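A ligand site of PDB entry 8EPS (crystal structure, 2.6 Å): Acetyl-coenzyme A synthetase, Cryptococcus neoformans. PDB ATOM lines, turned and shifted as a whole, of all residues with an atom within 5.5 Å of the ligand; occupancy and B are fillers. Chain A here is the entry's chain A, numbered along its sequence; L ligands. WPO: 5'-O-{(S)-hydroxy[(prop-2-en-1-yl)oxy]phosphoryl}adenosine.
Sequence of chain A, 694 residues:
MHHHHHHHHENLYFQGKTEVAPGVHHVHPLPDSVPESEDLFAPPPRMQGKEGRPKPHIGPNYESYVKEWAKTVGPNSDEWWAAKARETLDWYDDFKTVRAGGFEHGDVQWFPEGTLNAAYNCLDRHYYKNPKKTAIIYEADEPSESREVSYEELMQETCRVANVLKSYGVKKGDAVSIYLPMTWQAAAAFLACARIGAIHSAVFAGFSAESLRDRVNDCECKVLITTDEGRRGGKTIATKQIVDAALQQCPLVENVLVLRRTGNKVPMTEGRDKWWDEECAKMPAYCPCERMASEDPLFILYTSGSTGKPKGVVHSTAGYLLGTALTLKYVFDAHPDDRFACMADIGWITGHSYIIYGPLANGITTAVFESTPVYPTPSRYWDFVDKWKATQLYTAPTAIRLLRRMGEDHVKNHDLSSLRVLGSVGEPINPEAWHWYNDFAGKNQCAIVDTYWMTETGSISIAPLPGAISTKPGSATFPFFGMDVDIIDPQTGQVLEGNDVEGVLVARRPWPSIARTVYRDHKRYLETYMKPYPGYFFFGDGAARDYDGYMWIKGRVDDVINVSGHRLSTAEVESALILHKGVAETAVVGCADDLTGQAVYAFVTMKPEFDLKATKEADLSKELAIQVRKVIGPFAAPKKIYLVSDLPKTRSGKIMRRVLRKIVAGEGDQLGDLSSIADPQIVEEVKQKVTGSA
The side-chain hydroxyl (OG1) of Thr 455 is in hydrogen-bond range of an oxygen (O2P) of the ligand, 2.7 Å away. The backbone NH of Thr 455 lies within hydrogen-bond range of an oxygen (O2P) of the ligand, at 2.5 Å. The side-chain carboxylate of Asp 541 sits at hydrogen-bond distance from an oxygen (O2') of the ligand. A nitrogen (N7) of the ligand sits at hydrogen-bond distance from the backbone NH (N) of Gly 426, at 3.4 Å. The backbone carbonyl oxygen (O) of Thr 451 lies within hydrogen-bond range of a nitrogen (N6) of the ligand, at 3.2 Å. The side-chain sulfur (SD) of Met 454 is in hydrogen-bond range of an oxygen (O3') of the ligand (3.1 Å). The side-chain carboxylate (OD1) of Asp 450 sits at hydrogen-bond distance from a nitrogen (N6) of the ligand (2.9 Å). NE1 of Trp 348 is in hydrogen-bond range of O1P of the ligand, 3.1 Å away.
The backbone carbonyl oxygen (O) of Ser 424 sits at hydrogen-bond distance from the side-chain hydroxyl (OG1) of Thr 451 (2.9 Å). The guanidinium group (NH1) of Arg 556 lies within hydrogen-bond range of the backbone carbonyl oxygen (O) of Phe 539, 3.4 Å away.
A nitrogen (N1) of the ligand lies close to the backbone carbonyl oxygen (O) of Glu 427. The backbone nitrogen (N) of Pro 428 lies close to a nitrogen (N3) of the ligand (3.4 Å). Ile 349 touches the ligand (CG2 to C1P, 3.2 Å). Val 425 touches the ligand. CA of Tyr 452 touches N6 of the ligand (3.5 Å). Trp 453 touches the ligand. CG2 of Ile 553 touches C2 of the ligand, 3.6 Å away. CD of Arg 556 touches O2' of the ligand, 3.3 Å away. Hydrophobic or aromatic side chains within 4 Å of the ligand: Trp 348, Ile 349, Val 425, Pro 428, Tyr 452, Trp 453, Met 454 and Ile 553. 15 residues have an atom within 4 Å of the ligand: Trp 348, Ile 349, Val 425, Gly 426, Glu 427, Pro 428, Asp 450, Thr 451, Tyr 452, Trp 453, Met 454, Thr 455, Asp 541, Ile 553 and Arg 556.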
ATOM      1  N   TRP A 348      28.552   8.929  22.578  1.00  0.00           N
ATOM      2  CA  TRP A 348      27.274   8.246  22.437  1.00  0.00           C
ATOM      3  C   TRP A 348      27.448   7.084  21.471  1.00  0.00           C
ATOM      4  O   TRP A 348      28.264   7.139  20.544  1.00  0.00           O
ATOM      5  CB  TRP A 348      26.205   9.217  21.924  1.00  0.00           C
ATOM      6  CG  TRP A 348      24.784   8.747  21.998  1.00  0.00           C
ATOM      7  CD1 TRP A 348      24.288   7.719  22.741  1.00  0.00           C
ATOM      8  CD2 TRP A 348      23.663   9.301  21.295  1.00  0.00           C
ATOM      9  NE1 TRP A 348      22.929   7.605  22.551  1.00  0.00           N
ATOM     10  CE2 TRP A 348      22.522   8.562  21.656  1.00  0.00           C
ATOM     11  CE3 TRP A 348      23.523  10.362  20.386  1.00  0.00           C
ATOM     12  CZ2 TRP A 348      21.253   8.848  21.151  1.00  0.00           C
ATOM     13  CZ3 TRP A 348      22.261  10.633  19.887  1.00  0.00           C
ATOM     14  CH2 TRP A 348      21.141   9.880  20.270  1.00  0.00           C
ATOM     15  N   ILE A 349      26.683   6.015  21.694  1.00  0.00           N
ATOM     16  CA  ILE A 349      26.755   4.866  20.785  1.00  0.00           C
ATOM     17  C   ILE A 349      26.460   5.304  19.358  1.00  0.00           C
ATOM     18  O   ILE A 349      26.983   4.719  18.405  1.00  0.00           O
ATOM     19  CB  ILE A 349      25.791   3.748  21.250  1.00  0.00           C
ATOM     20  CG1 ILE A 349      25.997   2.474  20.428  1.00  0.00           C
ATOM     21  CG2 ILE A 349      24.345   4.198  21.127  1.00  0.00           C
ATOM     22  CD1 ILE A 349      27.278   1.742  20.749  1.00  0.00           C
ATOM     23  N   THR A 350      25.634   6.331  19.184  1.00  0.00           N
ATOM     24  CA  THR A 350      25.353   6.829  17.844  1.00  0.00           C
ATOM     25  C   THR A 350      26.623   7.281  17.140  1.00  0.00           C
ATOM     26  O   THR A 350      26.748   7.134  15.922  1.00  0.00           O
ATOM     27  CB  THR A 350      24.358   7.990  17.906  1.00  0.00           C
ATOM     28  OG1 THR A 350      23.189   7.585  18.627  1.00  0.00           O
ATOM     29  CG2 THR A 350      23.951   8.428  16.505  1.00  0.00           C
ATOM     30  N   SER A 424      16.473  10.439  12.154  1.00  0.00           N
ATOM     31  CA  SER A 424      16.192  10.815  13.531  1.00  0.00           C
ATOM     32  C   SER A 424      16.542   9.646  14.442  1.00  0.00           C
ATOM     33  O   SER A 424      16.359   8.480  14.065  1.00  0.00           O
ATOM     34  CB  SER A 424      14.727  11.212  13.714  1.00  0.00           C
ATOM     35  OG  SER A 424      14.462  11.590  15.048  1.00  0.00           O
ATOM     36  N   VAL A 425      17.039   9.943  15.640  1.00  0.00           N
ATOM     37  CA  VAL A 425      17.537   8.901  16.526  1.00  0.00           C
ATOM     38  C   VAL A 425      17.584   9.456  17.945  1.00  0.00           C
ATOM     39  O   VAL A 425      17.929  10.620  18.154  1.00  0.00           O
ATOM     40  CB  VAL A 425      18.921   8.387  16.069  1.00  0.00           C
ATOM     41  CG1 VAL A 425      19.866   9.554  15.832  1.00  0.00           C
ATOM     42  CG2 VAL A 425      19.498   7.431  17.092  1.00  0.00           C
ATOM     43  N   GLY A 426      17.244   8.603  18.919  1.00  0.00           N
ATOM     44  CA  GLY A 426      17.429   8.902  20.333  1.00  0.00           C
ATOM     45  C   GLY A 426      16.146   8.857  21.137  1.00  0.00           C
ATOM     46  O   GLY A 426      16.180   8.572  22.335  1.00  0.00           O
ATOM     47  N   GLU A 427      15.015   9.125  20.500  1.00  0.00           N
ATOM     48  CA  GLU A 427      13.724   9.163  21.164  1.00  0.00           C
ATOM     49  C   GLU A 427      12.606   9.162  20.143  1.00  0.00           C
ATOM     50  O   GLU A 427      12.874   9.296  18.940  1.00  0.00           O
ATOM     51  CB  GLU A 427      13.610  10.404  22.063  1.00  0.00           C
ATOM     52  CG  GLU A 427      13.877  10.156  23.538  1.00  0.00           C
ATOM     53  CD  GLU A 427      13.512  11.345  24.397  1.00  0.00           C
ATOM     54  OE1 GLU A 427      13.457  12.476  23.866  1.00  0.00           O
ATOM     55  OE2 GLU A 427      13.281  11.154  25.616  1.00  0.00           O
ATOM     56  N   PRO A 428      11.346   9.039  20.549  1.00  0.00           N
ATOM     57  CA  PRO A 428      10.246   9.227  19.602  1.00  0.00           C
ATOM     58  C   PRO A 428      10.270  10.648  19.050  1.00  0.00           C
ATOM     59  O   PRO A 428      10.517  11.609  19.786  1.00  0.00           O
ATOM     60  CB  PRO A 428       8.990   8.960  20.440  1.00  0.00           C
ATOM     61  CG  PRO A 428       9.474   8.224  21.658  1.00  0.00           C
ATOM     62  CD  PRO A 428      10.866   8.697  21.903  1.00  0.00           C
ATOM     63  N   ILE A 429      10.012  10.769  17.755  1.00  0.00           N
ATOM     64  CA  ILE A 429       9.973  12.068  17.092  1.00  0.00           C
ATOM     65  C   ILE A 429       8.506  12.450  16.904  1.00  0.00           C
ATOM     66  O   ILE A 429       7.748  11.732  16.252  1.00  0.00           O
ATOM     67  CB  ILE A 429      10.728  12.039  15.751  1.00  0.00           C
ATOM     68  CG1 ILE A 429      10.730  13.442  15.123  1.00  0.00           C
ATOM     69  CG2 ILE A 429      10.104  11.027  14.791  1.00  0.00           C
ATOM     70  CD1 ILE A 429      11.529  13.546  13.842  1.00  0.00           C
ATOM     71  N   ASP A 450      13.334   7.033  10.743  1.00  0.00           N
ATOM     72  CA  ASP A 450      13.249   7.079  12.194  1.00  0.00           C
ATOM     73  C   ASP A 450      13.905   5.808  12.727  1.00  0.00           C
ATOM     74  O   ASP A 450      13.282   4.745  12.731  1.00  0.00           O
ATOM     75  CB  ASP A 450      11.805   7.204  12.649  1.00  0.00           C
ATOM     76  CG  ASP A 450      11.671   7.519  14.118  1.00  0.00           C
ATOM     77  OD1 ASP A 450      12.699   7.853  14.757  1.00  0.00           O
ATOM     78  OD2 ASP A 450      10.539   7.447  14.640  1.00  0.00           O
ATOM     79  N   THR A 451      15.158   5.914  13.155  1.00  0.00           N
ATOM     80  CA  THR A 451      15.963   4.754  13.509  1.00  0.00           C
ATOM     81  C   THR A 451      15.848   4.487  15.002  1.00  0.00           C
ATOM     82  O   THR A 451      16.333   5.287  15.820  1.00  0.00           O
ATOM     83  CB  THR A 451      17.423   4.959  13.109  1.00  0.00           C
ATOM     84  OG1 THR A 451      17.957   6.081  13.813  1.00  0.00           O
ATOM     85  CG2 THR A 451      17.543   5.190  11.610  1.00  0.00           C
ATOM     86  N   TYR A 452      15.237   3.369  15.366  1.00  0.00           N
ATOM     87  CA  TYR A 452      15.105   2.951  16.756  1.00  0.00           C
ATOM     88  C   TYR A 452      16.115   1.854  17.070  1.00  0.00           C
ATOM     89  O   TYR A 452      16.224   0.868  16.327  1.00  0.00           O
ATOM     90  CB  TYR A 452      13.687   2.437  17.047  1.00  0.00           C
ATOM     91  CG  TYR A 452      13.605   1.675  18.346  1.00  0.00           C
ATOM     92  CD1 TYR A 452      13.436   2.340  19.561  1.00  0.00           C
ATOM     93  CD2 TYR A 452      13.702   0.287  18.370  1.00  0.00           C
ATOM     94  CE1 TYR A 452      13.373   1.645  20.749  1.00  0.00           C
ATOM     95  CE2 TYR A 452      13.627  -0.415  19.555  1.00  0.00           C
ATOM     96  CZ  TYR A 452      13.464   0.265  20.736  1.00  0.00           C
ATOM     97  OH  TYR A 452      13.394  -0.429  21.917  1.00  0.00           O
ATOM     98  N   TRP A 453      16.853   2.032  18.158  1.00  0.00           N
ATOM     99  CA  TRP A 453      17.789   1.029  18.644  1.00  0.00           C
ATOM    100  C   TRP A 453      18.309   1.504  19.994  1.00  0.00           C
ATOM    101  O   TRP A 453      17.883   2.537  20.517  1.00  0.00           O
ATOM    102  CB  TRP A 453      18.918   0.779  17.639  1.00  0.00           C
ATOM    103  CG  TRP A 453      19.690   1.990  17.210  1.00  0.00           C
ATOM    104  CD1 TRP A 453      19.200   3.081  16.539  1.00  0.00           C
ATOM    105  CD2 TRP A 453      21.087   2.232  17.382  1.00  0.00           C
ATOM    106  NE1 TRP A 453      20.207   3.979  16.298  1.00  0.00           N
ATOM    107  CE2 TRP A 453      21.376   3.489  16.806  1.00  0.00           C
ATOM    108  CE3 TRP A 453      22.128   1.513  17.975  1.00  0.00           C
ATOM    109  CZ2 TRP A 453      22.652   4.035  16.819  1.00  0.00           C
ATOM    110  CZ3 TRP A 453      23.404   2.059  17.987  1.00  0.00           C
ATOM    111  CH2 TRP A 453      23.651   3.302  17.408  1.00  0.00           C
ATOM    112  N   MET A 454      19.234   0.724  20.556  1.00  0.00           N
ATOM    113  CA  MET A 454      19.800   1.031  21.868  1.00  0.00           C
ATOM    114  C   MET A 454      21.300   0.777  21.837  1.00  0.00           C
ATOM    115  O   MET A 454      21.837   0.177  20.897  1.00  0.00           O
ATOM    116  CB  MET A 454      19.165   0.183  22.973  1.00  0.00           C
ATOM    117  CG  MET A 454      17.664   0.059  22.890  1.00  0.00           C
ATOM    118  SD  MET A 454      16.970  -0.676  24.387  1.00  0.00           S
ATOM    119  CE  MET A 454      17.876  -2.223  24.447  1.00  0.00           C
ATOM    120  N   THR A 455      21.980   1.234  22.882  1.00  0.00           N
ATOM    121  CA  THR A 455      23.395   0.932  23.028  1.00  0.00           C
ATOM    122  C   THR A 455      23.626  -0.579  23.056  1.00  0.00           C
ATOM    123  O   THR A 455      24.654  -1.052  22.565  1.00  0.00           O
ATOM    124  CB  THR A 455      23.935   1.572  24.311  1.00  0.00           C
ATOM    125  OG1 THR A 455      23.681   2.991  24.287  1.00  0.00           O
ATOM    126  CG2 THR A 455      25.429   1.340  24.439  1.00  0.00           C
ATOM    127  N   GLU A 456      22.683  -1.333  23.614  1.00  0.00           N
ATOM    128  CA  GLU A 456      22.829  -2.776  23.740  1.00  0.00           C
ATOM    129  C   GLU A 456      22.503  -3.532  22.454  1.00  0.00           C
ATOM    130  O   GLU A 456      22.740  -4.742  22.393  1.00  0.00           O
ATOM    131  CB  GLU A 456      21.948  -3.304  24.872  1.00  0.00           C
ATOM    132  CG  GLU A 456      22.309  -2.765  26.252  1.00  0.00           C
ATOM    133  CD  GLU A 456      21.643  -1.446  26.561  1.00  0.00           C
ATOM    134  OE1 GLU A 456      21.375  -0.673  25.623  1.00  0.00           O
ATOM    135  OE2 GLU A 456      21.377  -1.177  27.766  1.00  0.00           O
ATOM    136  N   ALA A 476       8.890   4.093  13.360  1.00  0.00           N
ATOM    137  CA  ALA A 476      10.122   3.454  12.904  1.00  0.00           C
ATOM    138  C   ALA A 476       9.868   2.429  11.799  1.00  0.00           C
ATOM    139  O   ALA A 476      10.830   1.983  11.167  1.00  0.00           O
ATOM    140  CB  ALA A 476      10.827   2.781  14.080  1.00  0.00           C
ATOM    141  N   PHE A 539      13.861  -4.936  25.408  1.00  0.00           N
ATOM    142  CA  PHE A 539      14.388  -3.601  25.135  1.00  0.00           C
ATOM    143  C   PHE A 539      14.080  -2.635  26.274  1.00  0.00           C
ATOM    144  O   PHE A 539      14.934  -1.822  26.660  1.00  0.00           O
ATOM    145  CB  PHE A 539      13.792  -3.044  23.836  1.00  0.00           C
ATOM    146  CG  PHE A 539      14.197  -3.795  22.600  1.00  0.00           C
ATOM    147  CD1 PHE A 539      13.452  -4.883  22.167  1.00  0.00           C
ATOM    148  CD2 PHE A 539      15.279  -3.389  21.850  1.00  0.00           C
ATOM    149  CE1 PHE A 539      13.819  -5.573  21.026  1.00  0.00           C
ATOM    150  CE2 PHE A 539      15.652  -4.072  20.704  1.00  0.00           C
ATOM    151  CZ  PHE A 539      14.915  -5.167  20.291  1.00  0.00           C
ATOM    152  N   ASP A 541      11.022  -0.764  26.054  1.00  0.00           N
ATOM    153  CA  ASP A 541      10.133   0.215  25.453  1.00  0.00           C
ATOM    154  C   ASP A 541       8.768  -0.412  25.191  1.00  0.00           C
ATOM    155  O   ASP A 541       8.652  -1.604  24.914  1.00  0.00           O
ATOM    156  CB  ASP A 541      10.688   0.726  24.120  1.00  0.00           C
ATOM    157  CG  ASP A 541      12.047   1.352  24.263  1.00  0.00           C
ATOM    158  OD1 ASP A 541      12.135   2.501  24.745  1.00  0.00           O
ATOM    159  OD2 ASP A 541      13.031   0.676  23.904  1.00  0.00           O
ATOM    160  N   ILE A 553       7.118   2.969  18.394  1.00  0.00           N
ATOM    161  CA  ILE A 553       7.791   2.964  19.687  1.00  0.00           C
ATOM    162  C   ILE A 553       7.254   4.143  20.488  1.00  0.00           C
ATOM    163  O   ILE A 553       7.507   5.299  20.148  1.00  0.00           O
ATOM    164  CB  ILE A 553       9.319   3.047  19.521  1.00  0.00           C
ATOM    165  CG1 ILE A 553       9.815   1.960  18.556  1.00  0.00           C
ATOM    166  CG2 ILE A 553      10.002   2.912  20.881  1.00  0.00           C
ATOM    167  CD1 ILE A 553       9.474   0.546  18.981  1.00  0.00           C
ATOM    168  N   GLY A 555       7.669   4.891  23.858  1.00  0.00           N
ATOM    169  CA  GLY A 555       8.439   5.430  24.960  1.00  0.00           C
ATOM    170  C   GLY A 555       8.929   4.364  25.908  1.00  0.00           C
ATOM    171  O   GLY A 555       8.709   3.165  25.675  1.00  0.00           O
ATOM    172  N   ARG A 556       9.591   4.763  26.995  1.00  0.00           N
ATOM    173  CA  ARG A 556      10.096   3.810  27.962  1.00  0.00           C
ATOM    174  C   ARG A 556       8.961   3.231  28.795  1.00  0.00           C
ATOM    175  O   ARG A 556       8.045   3.953  29.217  1.00  0.00           O
ATOM    176  CB  ARG A 556      11.131   4.466  28.873  1.00  0.00           C
ATOM    177  CG  ARG A 556      12.406   4.912  28.163  1.00  0.00           C
ATOM    178  CD  ARG A 556      13.290   3.721  27.777  1.00  0.00           C
ATOM    179  NE  ARG A 556      13.789   3.008  28.941  1.00  0.00           N
ATOM    180  CZ  ARG A 556      14.524   1.906  28.894  1.00  0.00           C
ATOM    181  NH1 ARG A 556      14.872   1.358  27.736  1.00  0.00           N
ATOM    182  NH2 ARG A 556      14.920   1.329  30.024  1.00  0.00           N
ATOM    183  N   SER A 652      23.273  13.373  25.130  1.00  0.00           N
ATOM    184  CA  SER A 652      22.850  12.830  23.849  1.00  0.00           C
ATOM    185  C   SER A 652      21.566  13.491  23.348  1.00  0.00           C
ATOM    186  O   SER A 652      21.403  13.686  22.145  1.00  0.00           O
ATOM    187  CB  SER A 652      22.651  11.313  23.969  1.00  0.00           C
ATOM    188  OG  SER A 652      21.706  11.002  24.978  1.00  0.00           O
HETATM  189  O2' WPO L   1      13.909   4.322  24.576  1.00  0.00           O
HETATM  190  C2' WPO L   1      14.393   4.118  23.263  1.00  0.00           C
HETATM  191  C1' WPO L   1      14.983   5.407  22.706  1.00  0.00           C
HETATM  192  O4' WPO L   1      16.370   5.408  23.057  1.00  0.00           O
HETATM  193  C4' WPO L   1      16.661   4.203  23.802  1.00  0.00           C
HETATM  194  C5' WPO L   1      18.097   3.800  23.619  1.00  0.00           C
HETATM  195  O5' WPO L   1      18.960   4.728  24.304  1.00  0.00           O
HETATM  196  P   WPO L   1      20.476   4.690  23.784  1.00  0.00           P
HETATM  197  O1P WPO L   1      21.207   5.820  24.398  1.00  0.00           O
HETATM  198  O2P WPO L   1      20.990   3.300  23.908  1.00  0.00           O
HETATM  199  O3P WPO L   1      20.154   4.983  22.253  1.00  0.00           O
HETATM  200  C1P WPO L   1      21.145   4.727  21.256  1.00  0.00           C
HETATM  201  C2P WPO L   1      20.437   4.485  19.971  1.00  0.00           C
HETATM  202  C3P WPO L   1      19.592   5.320  19.433  1.00  0.00           C
HETATM  203  C3' WPO L   1      15.623   3.214  23.280  1.00  0.00           C
HETATM  204  O3' WPO L   1      15.561   2.079  24.129  1.00  0.00           O
HETATM  205  N9  WPO L   1      14.893   5.525  21.250  1.00  0.00           N
HETATM  206  C8  WPO L   1      15.934   5.463  20.353  1.00  0.00           C
HETATM  207  N7  WPO L   1      15.559   5.598  19.100  1.00  0.00           N
HETATM  208  C5  WPO L   1      14.177   5.757  19.180  1.00  0.00           C
HETATM  209  C4  WPO L   1      13.758   5.713  20.503  1.00  0.00           C
HETATM  210  N3  WPO L   1      12.497   5.829  20.935  1.00  0.00           N
HETATM  211  C2  WPO L   1      11.650   6.002  19.926  1.00  0.00           C
HETATM  212  N1  WPO L   1      11.913   6.070  18.614  1.00  0.00           N
HETATM  213  C6  WPO L   1      13.193   5.945  18.191  1.00  0.00           C
HETATM  214  N6  WPO L   1      13.446   6.012  16.889  1.00  0.00           N
